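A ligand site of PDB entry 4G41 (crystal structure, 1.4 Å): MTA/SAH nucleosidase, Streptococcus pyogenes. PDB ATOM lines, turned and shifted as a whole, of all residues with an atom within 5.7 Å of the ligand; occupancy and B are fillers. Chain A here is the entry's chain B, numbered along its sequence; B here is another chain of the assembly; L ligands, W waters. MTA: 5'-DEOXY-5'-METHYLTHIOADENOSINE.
An oxygen (O3') of the ligand lies within hydrogen-bond range of the side-chain carboxylate of Glu 179. An oxygen (O2') of the ligand lies within hydrogen-bond range of the backbone NH of Met 178, at 2.8 Å. The backbone NH (N) of Val 157 sits at hydrogen-bond distance from a nitrogen (N1) of the ligand (2.9 Å). O of Val 157 is in hydrogen-bond range of N6 of the ligand, 3.1 Å away. The side-chain carboxylate (OD1) of Asp 202 is in hydrogen-bond range of a nitrogen (N6) of the ligand, 3.0 Å away. An oxygen (O4') of the ligand lies within hydrogen-bond range of the side-chain hydroxyl of Ser 81, at 3.3 Å. The side-chain hydroxyl (OG) of Ser 201 is in hydrogen-bond range of a nitrogen (N7) of the ligand (3.4 Å). The backbone NH of Gly 83 lies within hydrogen-bond range of a nitrogen (N7) of the ligand, at 3.4 Å.
The side-chain carboxylate of Glu 177 lies within hydrogen-bond range of the backbone NH of Glu 179 (3.2 Å). The side-chain carboxylate (OE2) of Glu 179 sits at hydrogen-bond distance from the backbone NH (N) of Gly 56. OG of Ser 201 sits at hydrogen-bond distance from OD2 of Asp 202 (2.8 Å). O of Ser 81 lies within hydrogen-bond range of NH1 of Arg 198, 2.7 Å away. N of Ser 81 sits at hydrogen-bond distance from OE2 of Glu 17 (2.8 Å). OE2 of Glu 177 lies within salt-bridge range of NE of Arg 198 (3.0 Å). The backbone NH (N) of Ser 201 is in hydrogen-bond range of the backbone carbonyl oxygen (O) of Ala 82 (2.8 Å). The backbone NH of Met 14 lies within hydrogen-bond range of the side-chain carboxylate of Glu 17, 2.9 Å away.
Residues that only touch the ligand: Ala 13 (3.4 Å), Met 14 (3.4 Å), Val 55 (3.7 Å), Ala 82 (3.4 Å), Ser 155 (3.5 Å), Phe 156 (3.4 Å), Val 176 (3.9 Å), Glu 177 (3.3 Å), Arg 198 (3.5 Å), Phe 212 (3.4 Å) and Phe 110 of chain B (3.5 Å). Hydrophobic or aromatic side chains that line the ligand: Ala 13, Met 14, Val 55, Phe 156, Val 157, Val 176, Met 178, Phe 212 and Phe 110 of chain B. The nearest printed residue that does not touch the ligand is Ala 204 (4.05 Å).
Water W1 lies within hydrogen-bond range of the side-chain carboxylate (OE2) of Glu 17, an oxygen (O3') of the ligand, the guanidinium group (NH1) of Arg 198 and the side-chain carboxylate (OE1) of Glu 179.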
ATOM      1  N   ALA A  13      22.838 -26.335 -25.628  1.00  0.00           N
ATOM      2  CA  ALA A  13      23.903 -26.254 -26.641  1.00  0.00           C
ATOM      3  C   ALA A  13      25.288 -26.232 -26.075  1.00  0.00           C
ATOM      4  O   ALA A  13      26.225 -26.810 -26.712  1.00  0.00           O
ATOM      5  CB  ALA A  13      23.739 -24.988 -27.483  1.00  0.00           C
ATOM      6  N   MET A  14      25.479 -25.538 -24.912  1.00  0.00           N
ATOM      7  CA  MET A  14      26.842 -25.233 -24.450  1.00  0.00           C
ATOM      8  C   MET A  14      26.963 -25.689 -22.974  1.00  0.00           C
ATOM      9  O   MET A  14      25.980 -25.845 -22.190  1.00  0.00           O
ATOM     10  CB  MET A  14      27.036 -23.735 -24.556  1.00  0.00           C
ATOM     11  CG  MET A  14      27.177 -23.287 -26.019  1.00  0.00           C
ATOM     12  SD  MET A  14      27.231 -21.516 -26.201  1.00  0.00           S
ATOM     13  CE  MET A  14      25.588 -21.117 -25.633  1.00  0.00           C
ATOM     14  N   GLU A  17      25.213 -24.085 -20.078  1.00  0.00           N
ATOM     15  CA  GLU A  17      23.744 -24.258 -20.020  1.00  0.00           C
ATOM     16  C   GLU A  17      23.354 -25.659 -19.418  1.00  0.00           C
ATOM     17  O   GLU A  17      22.147 -25.905 -19.192  1.00  0.00           O
ATOM     18  CB  GLU A  17      23.175 -24.083 -21.451  1.00  0.00           C
ATOM     19  CG  GLU A  17      23.428 -22.655 -21.946  1.00  0.00           C
ATOM     20  CD  GLU A  17      23.256 -22.572 -23.473  1.00  0.00           C
ATOM     21  OE1 GLU A  17      23.591 -23.526 -24.168  1.00  0.00           O
ATOM     22  OE2 GLU A  17      22.836 -21.492 -24.023  1.00  0.00           O
ATOM     23  N   VAL A  55      26.320 -26.091 -30.746  1.00  0.00           N
ATOM     24  CA  VAL A  55      25.435 -25.005 -31.217  1.00  0.00           C
ATOM     25  C   VAL A  55      24.837 -25.271 -32.573  1.00  0.00           C
ATOM     26  O   VAL A  55      25.509 -25.898 -33.461  1.00  0.00           O
ATOM     27  CB  VAL A  55      26.310 -23.727 -31.320  1.00  0.00           C
ATOM     28  CG1 VAL A  55      25.606 -22.588 -32.082  1.00  0.00           C
ATOM     29  CG2 VAL A  55      26.757 -23.240 -29.962  1.00  0.00           C
ATOM     30  N   GLY A  56      23.594 -24.829 -32.717  1.00  0.00           N
ATOM     31  CA  GLY A  56      22.981 -24.728 -34.037  1.00  0.00           C
ATOM     32  C   GLY A  56      21.987 -25.821 -34.425  1.00  0.00           C
ATOM     33  O   GLY A  56      21.772 -26.781 -33.623  1.00  0.00           O
ATOM     34  N   SER A  81      20.547 -19.994 -23.235  1.00  0.00           N
ATOM     35  CA  SER A  81      20.625 -18.532 -23.383  1.00  0.00           C
ATOM     36  C   SER A  81      19.936 -18.110 -24.659  1.00  0.00           C
ATOM     37  O   SER A  81      19.849 -18.871 -25.625  1.00  0.00           O
ATOM     38  CB  SER A  81      22.120 -18.085 -23.400  1.00  0.00           C
ATOM     39  OG  SER A  81      22.825 -18.665 -24.512  1.00  0.00           O
ATOM     40  N   ALA A  82      19.578 -16.829 -24.725  1.00  0.00           N
ATOM     41  CA  ALA A  82      19.021 -16.282 -25.942  1.00  0.00           C
ATOM     42  C   ALA A  82      19.246 -14.776 -25.932  1.00  0.00           C
ATOM     43  O   ALA A  82      19.559 -14.163 -24.888  1.00  0.00           O
ATOM     44  CB  ALA A  82      17.495 -16.612 -26.087  1.00  0.00           C
ATOM     45  N   GLY A  83      18.996 -14.194 -27.089  1.00  0.00           N
ATOM     46  CA  GLY A  83      19.067 -12.705 -27.227  1.00  0.00           C
ATOM     47  C   GLY A  83      17.656 -12.120 -27.120  1.00  0.00           C
ATOM     48  O   GLY A  83      16.729 -12.517 -27.842  1.00  0.00           O
ATOM     49  N   SER A 155      22.257 -18.327 -36.971  1.00  0.00           N
ATOM     50  CA  SER A 155      23.114 -17.119 -36.831  1.00  0.00           C
ATOM     51  C   SER A 155      22.996 -16.594 -35.419  1.00  0.00           C
ATOM     52  O   SER A 155      21.907 -16.691 -34.802  1.00  0.00           O
ATOM     53  CB  SER A 155      22.567 -16.012 -37.737  1.00  0.00           C
ATOM     54  OG  SER A 155      22.898 -16.350 -39.101  1.00  0.00           O
ATOM     55  N   PHE A 156      24.113 -16.008 -34.925  1.00  0.00           N
ATOM     56  CA  PHE A 156      24.091 -15.314 -33.668  1.00  0.00           C
ATOM     57  C   PHE A 156      23.682 -13.875 -34.008  1.00  0.00           C
ATOM     58  O   PHE A 156      24.375 -13.171 -34.825  1.00  0.00           O
ATOM     59  CB  PHE A 156      25.489 -15.345 -33.053  1.00  0.00           C
ATOM     60  CG  PHE A 156      25.613 -14.522 -31.801  1.00  0.00           C
ATOM     61  CD1 PHE A 156      25.002 -14.973 -30.582  1.00  0.00           C
ATOM     62  CD2 PHE A 156      26.280 -13.285 -31.824  1.00  0.00           C
ATOM     63  CE1 PHE A 156      25.092 -14.220 -29.412  1.00  0.00           C
ATOM     64  CE2 PHE A 156      26.407 -12.550 -30.632  1.00  0.00           C
ATOM     65  CZ  PHE A 156      25.849 -12.970 -29.409  1.00  0.00           C
ATOM     66  N   VAL A 157      22.557 -13.424 -33.484  1.00  0.00           N
ATOM     67  CA  VAL A 157      21.941 -12.146 -33.889  1.00  0.00           C
ATOM     68  C   VAL A 157      22.628 -11.020 -33.103  1.00  0.00           C
ATOM     69  O   VAL A 157      22.603 -10.966 -31.856  1.00  0.00           O
ATOM     70  CB  VAL A 157      20.437 -12.129 -33.631  1.00  0.00           C
ATOM     71  CG1 VAL A 157      19.852 -10.786 -34.116  1.00  0.00           C
ATOM     72  CG2 VAL A 157      19.765 -13.258 -34.361  1.00  0.00           C
ATOM     73  N   ALA A 158      23.296 -10.113 -33.873  1.00  0.00           N
ATOM     74  CA  ALA A 158      24.061  -9.020 -33.256  1.00  0.00           C
ATOM     75  C   ALA A 158      24.060  -7.834 -34.181  1.00  0.00           C
ATOM     76  O   ALA A 158      24.939  -7.652 -35.044  1.00  0.00           O
ATOM     77  CB  ALA A 158      25.506  -9.513 -32.975  1.00  0.00           C
ATOM     78  N   VAL A 176      15.657 -14.547 -29.537  1.00  0.00           N
ATOM     79  CA  VAL A 176      16.210 -15.301 -30.663  1.00  0.00           C
ATOM     80  C   VAL A 176      17.333 -16.229 -30.205  1.00  0.00           C
ATOM     81  O   VAL A 176      18.106 -15.883 -29.283  1.00  0.00           O
ATOM     82  CB  VAL A 176      16.771 -14.327 -31.758  1.00  0.00           C
ATOM     83  CG1 VAL A 176      15.642 -13.564 -32.382  1.00  0.00           C
ATOM     84  CG2 VAL A 176      17.878 -13.364 -31.211  1.00  0.00           C
ATOM     85  N   GLU A 177      17.397 -17.362 -30.855  1.00  0.00           N
ATOM     86  CA  GLU A 177      18.467 -18.324 -30.516  1.00  0.00           C
ATOM     87  C   GLU A 177      18.711 -19.260 -31.702  1.00  0.00           C
ATOM     88  O   GLU A 177      18.247 -18.993 -32.826  1.00  0.00           O
ATOM     89  CB  GLU A 177      18.217 -19.042 -29.132  1.00  0.00           C
ATOM     90  CG  GLU A 177      16.711 -19.280 -28.863  1.00  0.00           C
ATOM     91  CD  GLU A 177      16.193 -20.577 -29.472  1.00  0.00           C
ATOM     92  OE1 GLU A 177      16.557 -20.909 -30.636  1.00  0.00           O
ATOM     93  OE2 GLU A 177      15.450 -21.341 -28.760  1.00  0.00           O
ATOM     94  N   MET A 178      19.552 -20.283 -31.513  1.00  0.00           N
ATOM     95  CA  MET A 178      20.085 -21.094 -32.637  1.00  0.00           C
ATOM     96  C   MET A 178      19.667 -22.552 -32.596  1.00  0.00           C
ATOM     97  O   MET A 178      20.097 -23.315 -33.448  1.00  0.00           O
ATOM     98  CB  MET A 178      21.584 -20.924 -32.773  1.00  0.00           C
ATOM     99  CG  MET A 178      21.973 -19.450 -33.037  1.00  0.00           C
ATOM    100  SD  MET A 178      23.779 -19.182 -32.925  1.00  0.00           S
ATOM    101  CE  MET A 178      24.339 -20.100 -34.326  1.00  0.00           C
ATOM    102  N   GLU A 179      18.853 -22.924 -31.635  1.00  0.00           N
ATOM    103  CA  GLU A 179      18.427 -24.358 -31.547  1.00  0.00           C
ATOM    104  C   GLU A 179      16.914 -24.575 -31.345  1.00  0.00           C
ATOM    105  O   GLU A 179      16.467 -25.712 -31.662  1.00  0.00           O
ATOM    106  CB  GLU A 179      19.103 -25.178 -30.447  1.00  0.00           C
ATOM    107  CG  GLU A 179      20.644 -25.137 -30.535  1.00  0.00           C
ATOM    108  CD  GLU A 179      21.315 -23.818 -30.052  1.00  0.00           C
ATOM    109  OE1 GLU A 179      20.769 -23.212 -29.082  1.00  0.00           O
ATOM    110  OE2 GLU A 179      22.462 -23.564 -30.466  1.00  0.00           O
ATOM    111  N   ARG A 198      14.338 -20.295 -22.194  1.00  0.00           N
ATOM    112  CA  ARG A 198      15.601 -19.547 -22.360  1.00  0.00           C
ATOM    113  C   ARG A 198      15.711 -18.422 -21.331  1.00  0.00           C
ATOM    114  O   ARG A 198      14.669 -17.908 -20.924  1.00  0.00           O
ATOM    115  CB  ARG A 198      15.647 -18.877 -23.767  1.00  0.00           C
ATOM    116  CG  ARG A 198      15.643 -19.940 -24.943  1.00  0.00           C
ATOM    117  CD  ARG A 198      17.007 -20.663 -25.065  1.00  0.00           C
ATOM    118  NE  ARG A 198      17.064 -21.535 -26.257  1.00  0.00           N
ATOM    119  CZ  ARG A 198      18.221 -21.936 -26.782  1.00  0.00           C
ATOM    120  NH1 ARG A 198      19.354 -21.468 -26.299  1.00  0.00           N
ATOM    121  NH2 ARG A 198      18.198 -22.767 -27.810  1.00  0.00           N
ATOM    122  N   SER A 201      20.799 -13.614 -22.397  1.00  0.00           N
ATOM    123  CA  SER A 201      22.225 -13.317 -22.160  1.00  0.00           C
ATOM    124  C   SER A 201      22.561 -11.963 -22.731  1.00  0.00           C
ATOM    125  O   SER A 201      23.677 -11.467 -22.388  1.00  0.00           O
ATOM    126  CB  SER A 201      23.120 -14.382 -22.809  1.00  0.00           C
ATOM    127  OG  SER A 201      22.724 -14.591 -24.147  1.00  0.00           O
ATOM    128  N   ASP A 202      21.738 -11.398 -23.590  1.00  0.00           N
ATOM    129  CA  ASP A 202      22.123 -10.152 -24.315  1.00  0.00           C
ATOM    130  C   ASP A 202      20.842  -9.608 -24.952  1.00  0.00           C
ATOM    131  O   ASP A 202      19.737 -10.224 -24.785  1.00  0.00           O
ATOM    132  CB  ASP A 202      23.272 -10.385 -25.342  1.00  0.00           C
ATOM    133  CG  ASP A 202      22.904 -11.475 -26.331  1.00  0.00           C
ATOM    134  OD1 ASP A 202      22.145 -11.187 -27.278  1.00  0.00           O
ATOM    135  OD2 ASP A 202      23.334 -12.612 -26.046  1.00  0.00           O
ATOM    136  N   THR A 203      20.986  -8.453 -25.642  1.00  0.00           N
ATOM    137  CA  THR A 203      19.866  -7.882 -26.374  1.00  0.00           C
ATOM    138  C   THR A 203      20.110  -7.901 -27.890  1.00  0.00           C
ATOM    139  O   THR A 203      19.524  -7.103 -28.615  1.00  0.00           O
ATOM    140  CB  THR A 203      19.522  -6.468 -25.860  1.00  0.00           C
ATOM    141  OG1 THR A 203      20.707  -5.684 -25.895  1.00  0.00           O
ATOM    142  CG2 THR A 203      19.040  -6.560 -24.416  1.00  0.00           C
ATOM    143  N   ALA A 204      21.022  -8.743 -28.374  1.00  0.00           N
ATOM    144  CA  ALA A 204      21.257  -8.993 -29.830  1.00  0.00           C
ATOM    145  C   ALA A 204      21.692  -7.705 -30.487  1.00  0.00           C
ATOM    146  O   ALA A 204      21.430  -7.531 -31.662  1.00  0.00           O
ATOM    147  CB  ALA A 204      19.916  -9.496 -30.506  1.00  0.00           C
ATOM    148  N   ALA A 208      26.709  -7.690 -29.284  1.00  0.00           N
ATOM    149  CA  ALA A 208      26.114  -8.683 -28.393  1.00  0.00           C
ATOM    150  C   ALA A 208      27.084  -9.795 -27.991  1.00  0.00           C
ATOM    151  O   ALA A 208      26.844 -10.393 -26.923  1.00  0.00           O
ATOM    152  CB  ALA A 208      24.882  -9.339 -29.039  1.00  0.00           C
ATOM    153  N   PHE A 212      27.030 -11.281 -24.332  1.00  0.00           N
ATOM    154  CA  PHE A 212      26.876 -12.729 -24.159  1.00  0.00           C
ATOM    155  C   PHE A 212      28.020 -13.284 -23.337  1.00  0.00           C
ATOM    156  O   PHE A 212      27.798 -14.073 -22.380  1.00  0.00           O
ATOM    157  CB  PHE A 212      26.859 -13.347 -25.566  1.00  0.00           C
ATOM    158  CG  PHE A 212      26.941 -14.868 -25.548  1.00  0.00           C
ATOM    159  CD1 PHE A 212      25.782 -15.671 -25.686  1.00  0.00           C
ATOM    160  CD2 PHE A 212      28.182 -15.476 -25.440  1.00  0.00           C
ATOM    161  CE1 PHE A 212      25.910 -17.078 -25.697  1.00  0.00           C
ATOM    162  CE2 PHE A 212      28.362 -16.869 -25.415  1.00  0.00           C
ATOM    163  CZ  PHE A 212      27.183 -17.671 -25.548  1.00  0.00           C
ATOM    164  N   ILE A 216      26.670 -15.331 -20.147  1.00  0.00           N
ATOM    165  CA  ILE A 216      26.322 -16.706 -20.466  1.00  0.00           C
ATOM    166  C   ILE A 216      26.284 -17.597 -19.246  1.00  0.00           C
ATOM    167  O   ILE A 216      25.369 -18.449 -19.166  1.00  0.00           O
ATOM    168  CB  ILE A 216      27.277 -17.244 -21.577  1.00  0.00           C
ATOM    169  CG1 ILE A 216      26.923 -18.728 -21.951  1.00  0.00           C
ATOM    170  CG2 ILE A 216      28.796 -17.169 -21.289  1.00  0.00           C
ATOM    171  CD1 ILE A 216      25.468 -18.946 -22.377  1.00  0.00           C
ATOM    172  N   ALA B 107      27.901 -16.236 -37.420  1.00  0.00           N
ATOM    173  CA  ALA B 107      28.334 -16.110 -36.012  1.00  0.00           C
ATOM    174  C   ALA B 107      29.580 -15.214 -36.020  1.00  0.00           C
ATOM    175  O   ALA B 107      30.446 -15.344 -35.143  1.00  0.00           O
ATOM    176  CB  ALA B 107      28.589 -17.505 -35.441  1.00  0.00           C
ATOM    177  N   PHE B 110      31.362 -13.291 -32.993  1.00  0.00           N
ATOM    178  CA  PHE B 110      32.295 -13.994 -32.100  1.00  0.00           C
ATOM    179  C   PHE B 110      33.698 -14.123 -32.726  1.00  0.00           C
ATOM    180  O   PHE B 110      34.627 -14.591 -32.057  1.00  0.00           O
ATOM    181  CB  PHE B 110      31.778 -15.365 -31.739  1.00  0.00           C
ATOM    182  CG  PHE B 110      30.617 -15.332 -30.787  1.00  0.00           C
ATOM    183  CD1 PHE B 110      30.734 -14.754 -29.504  1.00  0.00           C
ATOM    184  CD2 PHE B 110      29.369 -15.867 -31.154  1.00  0.00           C
ATOM    185  CE1 PHE B 110      29.699 -14.776 -28.579  1.00  0.00           C
ATOM    186  CE2 PHE B 110      28.334 -15.867 -30.230  1.00  0.00           C
ATOM    187  CZ  PHE B 110      28.498 -15.292 -29.006  1.00  0.00           C
ATOM    188  N   ALA B 118      29.503 -22.020 -35.143  1.00  0.00           N
ATOM    189  CA  ALA B 118      30.274 -22.049 -33.895  1.00  0.00           C
ATOM    190  C   ALA B 118      30.672 -23.489 -33.598  1.00  0.00           C
ATOM    191  O   ALA B 118      29.866 -24.389 -33.723  1.00  0.00           O
ATOM    192  CB  ALA B 118      29.436 -21.503 -32.775  1.00  0.00           C
HETATM  193  CS  MTA L   1      27.802 -19.244 -29.451  1.00  0.00           C
HETATM  194  S5' MTA L   1      26.458 -19.065 -30.644  1.00  0.00           S
HETATM  195  C5' MTA L   1      25.120 -18.512 -29.612  1.00  0.00           C
HETATM  196  C4' MTA L   1      24.589 -19.661 -28.664  1.00  0.00           C
HETATM  197  O4' MTA L   1      23.808 -19.037 -27.603  1.00  0.00           O
HETATM  198  C2' MTA L   1      22.313 -19.732 -29.224  1.00  0.00           C
HETATM  199  O2' MTA L   1      21.127 -20.571 -29.229  1.00  0.00           O
HETATM  200  C3' MTA L   1      23.615 -20.536 -29.379  1.00  0.00           C
HETATM  201  O3' MTA L   1      23.545 -21.837 -28.746  1.00  0.00           O
HETATM  202  C1' MTA L   1      22.382 -18.913 -27.944  1.00  0.00           C
HETATM  203  N9  MTA L   1      22.189 -17.462 -28.139  1.00  0.00           N
HETATM  204  C8  MTA L   1      22.356 -16.631 -27.034  1.00  0.00           C
HETATM  205  N7  MTA L   1      22.215 -15.281 -27.411  1.00  0.00           N
HETATM  206  C5  MTA L   1      21.963 -15.332 -28.806  1.00  0.00           C
HETATM  207  C6  MTA L   1      21.749 -14.349 -29.854  1.00  0.00           C
HETATM  208  N6  MTA L   1      21.799 -12.997 -29.639  1.00  0.00           N
HETATM  209  N1  MTA L   1      21.512 -14.781 -31.090  1.00  0.00           N
HETATM  210  C2  MTA L   1      21.469 -16.075 -31.433  1.00  0.00           C
HETATM  211  N3  MTA L   1      21.642 -17.061 -30.536  1.00  0.00           N
HETATM  212  C4  MTA L   1      21.899 -16.709 -29.262  1.00  0.00           C
HETATM  213  O   HOH W   1      22.012 -22.196 -26.497  1.00  0.00           O
